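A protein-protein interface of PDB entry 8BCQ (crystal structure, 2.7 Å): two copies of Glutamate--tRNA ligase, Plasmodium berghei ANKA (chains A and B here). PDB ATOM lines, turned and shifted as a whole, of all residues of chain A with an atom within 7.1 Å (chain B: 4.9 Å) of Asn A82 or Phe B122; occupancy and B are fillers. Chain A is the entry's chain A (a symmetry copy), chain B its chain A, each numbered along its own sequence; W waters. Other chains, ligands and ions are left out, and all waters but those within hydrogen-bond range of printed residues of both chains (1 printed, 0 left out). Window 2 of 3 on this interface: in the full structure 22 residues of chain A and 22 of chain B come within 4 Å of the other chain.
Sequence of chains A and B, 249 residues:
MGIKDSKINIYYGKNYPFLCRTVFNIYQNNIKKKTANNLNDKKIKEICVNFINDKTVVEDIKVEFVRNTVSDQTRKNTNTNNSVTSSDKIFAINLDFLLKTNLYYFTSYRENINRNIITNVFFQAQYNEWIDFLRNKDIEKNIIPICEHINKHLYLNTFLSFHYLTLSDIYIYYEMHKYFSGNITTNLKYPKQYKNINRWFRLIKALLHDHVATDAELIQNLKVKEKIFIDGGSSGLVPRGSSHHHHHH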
ATOM      1  N   VAL A  63      -8.401 -10.886   7.584  1.00  0.00           N
ATOM      2  CA  VAL A  63      -9.776 -10.399   7.627  1.00  0.00           C
ATOM      3  C   VAL A  63     -10.031  -9.542   6.397  1.00  0.00           C
ATOM      4  O   VAL A  63      -9.293  -8.586   6.135  1.00  0.00           O
ATOM      5  CB  VAL A  63     -10.056  -9.601   8.911  1.00  0.00           C
ATOM      6  CG1 VAL A  63     -11.492  -9.108   8.919  1.00  0.00           C
ATOM      7  CG2 VAL A  63      -9.776 -10.454  10.131  1.00  0.00           C
ATOM      8  N   GLU A  64     -11.084  -9.875   5.659  1.00  0.00           N
ATOM      9  CA  GLU A  64     -11.465  -9.156   4.453  1.00  0.00           C
ATOM     10  C   GLU A  64     -12.820  -8.499   4.671  1.00  0.00           C
ATOM     11  O   GLU A  64     -13.775  -9.160   5.092  1.00  0.00           O
ATOM     12  CB  GLU A  64     -11.518 -10.098   3.247  1.00  0.00           C
ATOM     13  CG  GLU A  64     -11.959  -9.433   1.960  1.00  0.00           C
ATOM     14  CD  GLU A  64     -12.093 -10.417   0.817  1.00  0.00           C
ATOM     15  OE1 GLU A  64     -12.135 -11.637   1.085  1.00  0.00           O
ATOM     16  OE2 GLU A  64     -12.154  -9.971  -0.350  1.00  0.00           O
ATOM     17  N   PHE A  65     -12.899  -7.204   4.385  1.00  0.00           N
ATOM     18  CA  PHE A  65     -14.132  -6.441   4.529  1.00  0.00           C
ATOM     19  C   PHE A  65     -14.772  -6.273   3.156  1.00  0.00           C
ATOM     20  O   PHE A  65     -14.154  -5.719   2.241  1.00  0.00           O
ATOM     21  CB  PHE A  65     -13.860  -5.081   5.174  1.00  0.00           C
ATOM     22  CG  PHE A  65     -13.419  -5.171   6.609  1.00  0.00           C
ATOM     23  CD1 PHE A  65     -12.092  -5.408   6.929  1.00  0.00           C
ATOM     24  CD2 PHE A  65     -14.331  -5.015   7.641  1.00  0.00           C
ATOM     25  CE1 PHE A  65     -11.684  -5.491   8.247  1.00  0.00           C
ATOM     26  CE2 PHE A  65     -13.928  -5.096   8.960  1.00  0.00           C
ATOM     27  CZ  PHE A  65     -12.602  -5.334   9.262  1.00  0.00           C
ATOM     28  N   VAL A  66     -16.006  -6.750   3.018  1.00  0.00           N
ATOM     29  CA  VAL A  66     -16.734  -6.729   1.754  1.00  0.00           C
ATOM     30  C   VAL A  66     -17.843  -5.693   1.855  1.00  0.00           C
ATOM     31  O   VAL A  66     -18.668  -5.744   2.777  1.00  0.00           O
ATOM     32  CB  VAL A  66     -17.305  -8.116   1.412  1.00  0.00           C
ATOM     33  CG1 VAL A  66     -17.976  -8.091   0.052  1.00  0.00           C
ATOM     34  CG2 VAL A  66     -16.206  -9.170   1.454  1.00  0.00           C
ATOM     35  N   ARG A  67     -17.862  -4.756   0.913  1.00  0.00           N
ATOM     36  CA  ARG A  67     -18.856  -3.687   0.910  1.00  0.00           C
ATOM     37  C   ARG A  67     -19.515  -3.555  -0.458  1.00  0.00           C
ATOM     38  O   ARG A  67     -19.154  -4.256  -1.404  1.00  0.00           O
ATOM     39  CB  ARG A  67     -18.212  -2.360   1.318  1.00  0.00           C
ATOM     40  CG  ARG A  67     -17.559  -2.390   2.691  1.00  0.00           C
ATOM     41  CD  ARG A  67     -16.600  -1.228   2.882  1.00  0.00           C
ATOM     42  NE  ARG A  67     -15.701  -1.455   4.006  1.00  0.00           N
ATOM     43  CZ  ARG A  67     -14.645  -0.703   4.289  1.00  0.00           C
ATOM     44  NH1 ARG A  67     -14.327   0.347   3.551  1.00  0.00           N
ATOM     45  NH2 ARG A  67     -13.890  -1.017   5.336  1.00  0.00           N
ATOM     46  N   ASN A  82     -10.800  -4.643   0.654  1.00  0.00           N
ATOM     47  CA  ASN A  82      -9.857  -4.222   1.686  1.00  0.00           C
ATOM     48  C   ASN A  82      -9.680  -5.295   2.755  1.00  0.00           C
ATOM     49  O   ASN A  82     -10.653  -5.771   3.343  1.00  0.00           O
ATOM     50  CB  ASN A  82     -10.317  -2.914   2.329  1.00  0.00           C
ATOM     51  CG  ASN A  82      -9.942  -1.700   1.507  1.00  0.00           C
ATOM     52  OD1 ASN A  82      -8.858  -1.642   0.927  1.00  0.00           O
ATOM     53  ND2 ASN A  82     -10.840  -0.721   1.453  1.00  0.00           N
ATOM     54  N   SER A  83      -8.429  -5.667   3.011  1.00  0.00           N
ATOM     55  CA  SER A  83      -8.113  -6.726   3.952  1.00  0.00           C
ATOM     56  C   SER A  83      -7.080  -6.237   4.958  1.00  0.00           C
ATOM     57  O   SER A  83      -6.332  -5.288   4.706  1.00  0.00           O
ATOM     58  CB  SER A  83      -7.594  -7.979   3.236  1.00  0.00           C
ATOM     59  OG  SER A  83      -6.354  -7.723   2.603  1.00  0.00           O
ATOM     60  N   VAL A  84      -7.058  -6.896   6.116  1.00  0.00           N
ATOM     61  CA  VAL A  84      -6.088  -6.618   7.165  1.00  0.00           C
ATOM     62  C   VAL A  84      -5.526  -7.938   7.671  1.00  0.00           C
ATOM     63  O   VAL A  84      -6.104  -9.009   7.474  1.00  0.00           O
ATOM     64  CB  VAL A  84      -6.690  -5.820   8.344  1.00  0.00           C
ATOM     65  CG1 VAL A  84      -7.087  -4.418   7.906  1.00  0.00           C
ATOM     66  CG2 VAL A  84      -7.879  -6.566   8.935  1.00  0.00           C
ATOM     67  N   PHE A  91      -8.358  -9.449  17.059  1.00  0.00           N
ATOM     68  CA  PHE A  91      -9.504  -9.049  16.250  1.00  0.00           C
ATOM     69  C   PHE A  91     -10.828  -9.326  16.952  1.00  0.00           C
ATOM     70  O   PHE A  91     -11.845  -8.730  16.582  1.00  0.00           O
ATOM     71  CB  PHE A  91      -9.470  -9.748  14.887  1.00  0.00           C
ATOM     72  CG  PHE A  91     -10.530  -9.265  13.931  1.00  0.00           C
ATOM     73  CD1 PHE A  91     -10.467  -7.988  13.388  1.00  0.00           C
ATOM     74  CD2 PHE A  91     -11.588 -10.088  13.571  1.00  0.00           C
ATOM     75  CE1 PHE A  91     -11.440  -7.541  12.511  1.00  0.00           C
ATOM     76  CE2 PHE A  91     -12.562  -9.645  12.691  1.00  0.00           C
ATOM     77  CZ  PHE A  91     -12.489  -8.369  12.165  1.00  0.00           C
ATOM     78  N   ASN A  94     -12.306  -6.236  18.038  1.00  0.00           N
ATOM     79  CA  ASN A  94     -13.053  -5.546  16.992  1.00  0.00           C
ATOM     80  C   ASN A  94     -14.450  -6.132  16.835  1.00  0.00           C
ATOM     81  O   ASN A  94     -15.428  -5.390  16.680  1.00  0.00           O
ATOM     82  CB  ASN A  94     -12.294  -5.620  15.668  1.00  0.00           C
ATOM     83  CG  ASN A  94     -10.973  -4.881  15.710  1.00  0.00           C
ATOM     84  OD1 ASN A  94      -9.905  -5.490  15.654  1.00  0.00           O
ATOM     85  ND2 ASN A  94     -11.037  -3.557  15.800  1.00  0.00           N
ATOM     86  N   ILE B 118     -18.339  -0.155  10.470  1.00  0.00           N
ATOM     87  CA  ILE B 118     -17.444  -1.139   9.868  1.00  0.00           C
ATOM     88  C   ILE B 118     -16.183  -0.462   9.348  1.00  0.00           C
ATOM     89  O   ILE B 118     -15.086  -1.033   9.398  1.00  0.00           O
ATOM     90  CB  ILE B 118     -18.178  -1.915   8.761  1.00  0.00           C
ATOM     91  CG1 ILE B 118     -19.352  -2.684   9.358  1.00  0.00           C
ATOM     92  CG2 ILE B 118     -17.232  -2.871   8.048  1.00  0.00           C
ATOM     93  CD1 ILE B 118     -20.462  -2.927   8.386  1.00  0.00           C
ATOM     94  N   THR B 119     -16.315   0.760   8.832  1.00  0.00           N
ATOM     95  CA  THR B 119     -15.131   1.524   8.463  1.00  0.00           C
ATOM     96  C   THR B 119     -14.277   1.818   9.688  1.00  0.00           C
ATOM     97  O   THR B 119     -13.044   1.757   9.625  1.00  0.00           O
ATOM     98  CB  THR B 119     -15.539   2.819   7.760  1.00  0.00           C
ATOM     99  OG1 THR B 119     -16.356   2.507   6.624  1.00  0.00           O
ATOM    100  CG2 THR B 119     -14.311   3.581   7.291  1.00  0.00           C
ATOM    101  N   ASN B 120     -14.921   2.132  10.817  1.00  0.00           N
ATOM    102  CA  ASN B 120     -14.193   2.340  12.065  1.00  0.00           C
ATOM    103  C   ASN B 120     -13.446   1.077  12.477  1.00  0.00           C
ATOM    104  O   ASN B 120     -12.261   1.128  12.828  1.00  0.00           O
ATOM    105  CB  ASN B 120     -15.166   2.768  13.165  1.00  0.00           C
ATOM    106  CG  ASN B 120     -14.483   3.494  14.310  1.00  0.00           C
ATOM    107  OD1 ASN B 120     -15.140   4.159  15.108  1.00  0.00           O
ATOM    108  ND2 ASN B 120     -13.161   3.389  14.383  1.00  0.00           N
ATOM    109  N   VAL B 121     -14.127  -0.072  12.428  1.00  0.00           N
ATOM    110  CA  VAL B 121     -13.491  -1.336  12.788  1.00  0.00           C
ATOM    111  C   VAL B 121     -12.309  -1.620  11.873  1.00  0.00           C
ATOM    112  O   VAL B 121     -11.248  -2.068  12.325  1.00  0.00           O
ATOM    113  CB  VAL B 121     -14.524  -2.477  12.750  1.00  0.00           C
ATOM    114  CG1 VAL B 121     -13.835  -3.828  12.878  1.00  0.00           C
ATOM    115  CG2 VAL B 121     -15.557  -2.291  13.848  1.00  0.00           C
ATOM    116  N   PHE B 122     -12.470  -1.357  10.574  1.00  0.00           N
ATOM    117  CA  PHE B 122     -11.387  -1.597   9.627  1.00  0.00           C
ATOM    118  C   PHE B 122     -10.160  -0.759   9.963  1.00  0.00           C
ATOM    119  O   PHE B 122      -9.026  -1.247   9.884  1.00  0.00           O
ATOM    120  CB  PHE B 122     -11.866  -1.310   8.202  1.00  0.00           C
ATOM    121  CG  PHE B 122     -10.768  -1.323   7.177  1.00  0.00           C
ATOM    122  CD1 PHE B 122     -10.271  -2.521   6.687  1.00  0.00           C
ATOM    123  CD2 PHE B 122     -10.236  -0.137   6.696  1.00  0.00           C
ATOM    124  CE1 PHE B 122      -9.262  -2.534   5.740  1.00  0.00           C
ATOM    125  CE2 PHE B 122      -9.226  -0.145   5.752  1.00  0.00           C
ATOM    126  CZ  PHE B 122      -8.741  -1.344   5.274  1.00  0.00           C
ATOM    127  N   PHE B 123     -10.362   0.506  10.347  1.00  0.00           N
ATOM    128  CA  PHE B 123      -9.225   1.341  10.725  1.00  0.00           C
ATOM    129  C   PHE B 123      -8.509   0.787  11.949  1.00  0.00           C
ATOM    130  O   PHE B 123      -7.275   0.810  12.018  1.00  0.00           O
ATOM    131  CB  PHE B 123      -9.670   2.774  11.002  1.00  0.00           C
ATOM    132  CG  PHE B 123      -8.720   3.519  11.892  1.00  0.00           C
ATOM    133  CD1 PHE B 123      -7.496   3.951  11.408  1.00  0.00           C
ATOM    134  CD2 PHE B 123      -9.031   3.754  13.220  1.00  0.00           C
ATOM    135  CE1 PHE B 123      -6.609   4.618  12.226  1.00  0.00           C
ATOM    136  CE2 PHE B 123      -8.148   4.424  14.041  1.00  0.00           C
ATOM    137  CZ  PHE B 123      -6.935   4.857  13.544  1.00  0.00           C
ATOM    138  N   GLN B 124      -9.270   0.309  12.936  1.00  0.00           N
ATOM    139  CA  GLN B 124      -8.657  -0.191  14.163  1.00  0.00           C
ATOM    140  C   GLN B 124      -7.718  -1.353  13.870  1.00  0.00           C
ATOM    141  O   GLN B 124      -6.618  -1.428  14.429  1.00  0.00           O
ATOM    142  CB  GLN B 124      -9.744  -0.600  15.156  1.00  0.00           C
ATOM    143  CG  GLN B 124     -10.697   0.533  15.520  1.00  0.00           C
ATOM    144  CD  GLN B 124     -11.881   0.074  16.347  1.00  0.00           C
ATOM    145  OE1 GLN B 124     -12.090  -1.121  16.546  1.00  0.00           O
ATOM    146  NE2 GLN B 124     -12.667   1.028  16.833  1.00  0.00           N
ATOM    147  N   ALA B 125      -8.125  -2.260  12.977  1.00  0.00           N
ATOM    148  CA  ALA B 125      -7.230  -3.340  12.575  1.00  0.00           C
ATOM    149  C   ALA B 125      -6.008  -2.808  11.838  1.00  0.00           C
ATOM    150  O   ALA B 125      -4.937  -3.424  11.891  1.00  0.00           O
ATOM    151  CB  ALA B 125      -7.978  -4.349  11.709  1.00  0.00           C
ATOM    152  N   GLN B 126      -6.143  -1.673  11.149  1.00  0.00           N
ATOM    153  CA  GLN B 126      -4.990  -1.077  10.483  1.00  0.00           C
ATOM    154  C   GLN B 126      -4.013  -0.482  11.487  1.00  0.00           C
ATOM    155  O   GLN B 126      -2.795  -0.556  11.290  1.00  0.00           O
ATOM    156  CB  GLN B 126      -5.447  -0.017   9.484  1.00  0.00           C
ATOM    157  CG  GLN B 126      -5.992  -0.587   8.194  1.00  0.00           C
ATOM    158  CD  GLN B 126      -6.119   0.462   7.116  1.00  0.00           C
ATOM    159  OE1 GLN B 126      -6.420   1.622   7.397  1.00  0.00           O
ATOM    160  NE2 GLN B 126      -5.875   0.065   5.873  1.00  0.00           N
ATOM    161  N   PHE B 162      -7.001   6.300   5.510  1.00  0.00           N
ATOM    162  CA  PHE B 162      -8.117   7.103   4.978  1.00  0.00           C
ATOM    163  C   PHE B 162      -7.566   8.466   4.546  1.00  0.00           C
ATOM    164  O   PHE B 162      -6.511   8.529   3.896  1.00  0.00           O
ATOM    165  CB  PHE B 162      -9.227   7.152   6.003  1.00  0.00           C
ATOM    166  CG  PHE B 162      -9.784   5.806   6.352  1.00  0.00           C
ATOM    167  CD1 PHE B 162     -10.024   4.866   5.362  1.00  0.00           C
ATOM    168  CD2 PHE B 162     -10.053   5.470   7.667  1.00  0.00           C
ATOM    169  CE1 PHE B 162     -10.533   3.621   5.678  1.00  0.00           C
ATOM    170  CE2 PHE B 162     -10.562   4.228   7.988  1.00  0.00           C
ATOM    171  CZ  PHE B 162     -10.801   3.301   6.993  1.00  0.00           C
HETATM  172  O   HOH W   1     -11.715  -2.786  18.763  1.00  0.00           O
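The side-chain amide nitrogen of Asn A94 lies within hydrogen-bond range of the side-chain amide oxygen of Gln B124 (2.8 Å).
N of Phe A65 lies within hydrogen-bond range of O of Asn A82 (2.9 Å).
The side-chain amide nitrogen (ND2) of Asn B120 sits close to the side-chain amide nitrogen (NE2) of Gln B124, 3.4 Å away.
The backbone NH of Val A84 sits at hydrogen-bond distance from the backbone carbonyl oxygen of Val A63 (2.8 Å).
Among the printed residues, pairs that only touch across the chains: Phe A65 with Phe B122 (3.4 Å), Arg A67 with Phe B122 (3.5 Å), Val A84 with Ala B125 (3.6 Å), Asn A82 with Phe B122 (3.6 Å), Val A84 with Phe B122 (3.6 Å), Phe A65 with Ile B118 (3.6 Å), Asn A94 with Val B121 (3.7 Å) and Val A84 with Gln B126 (3.99 Å).
Of chain A, only Phe A65, Arg A67, Asn A82 and Val A84 come within 4 Å of Phe B122.
Printed residues of chain B within 4 Å of Asn A94: Val B121 and Gln B124.
Of the printed residues of chain A, Gln B124 touches Asn A94 (2.8 Å).
Of the printed residues of chain A, Val B121 touches Asn A94 (3.7 Å).
Printed residues of chain A within 4 Å of Gln B126: Val A84.
The nearest printed residue of chain B that does not touch Asn A82 is Gln B126 (6.0 Å).
The nearest printed residue of chain A that does not touch Gln B124 is Val A84 (6.7 Å).
Of the 10 printed residues of chain A, 5 touch a printed residue of chain B.
Printed residues of chain A that touch a printed residue of chain B: Phe A65, Arg A67, Asn A82, Val A84 and Asn A94.
Hydrophobic or aromatic side chains of chain A that line the printed part of chain B: Phe A65 and Val A84.
No position is printed for both chains.
Of the 9 pairs that touch across the chains among the printed residues, none has its exchanged pair printed and touching as well.
Water W1 lies within hydrogen-bond range of the side-chain amide oxygen (OE1) of Gln B124 (2.8 Å) and the side-chain amide nitrogen (ND2) of Asn A94 (3.1 Å).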
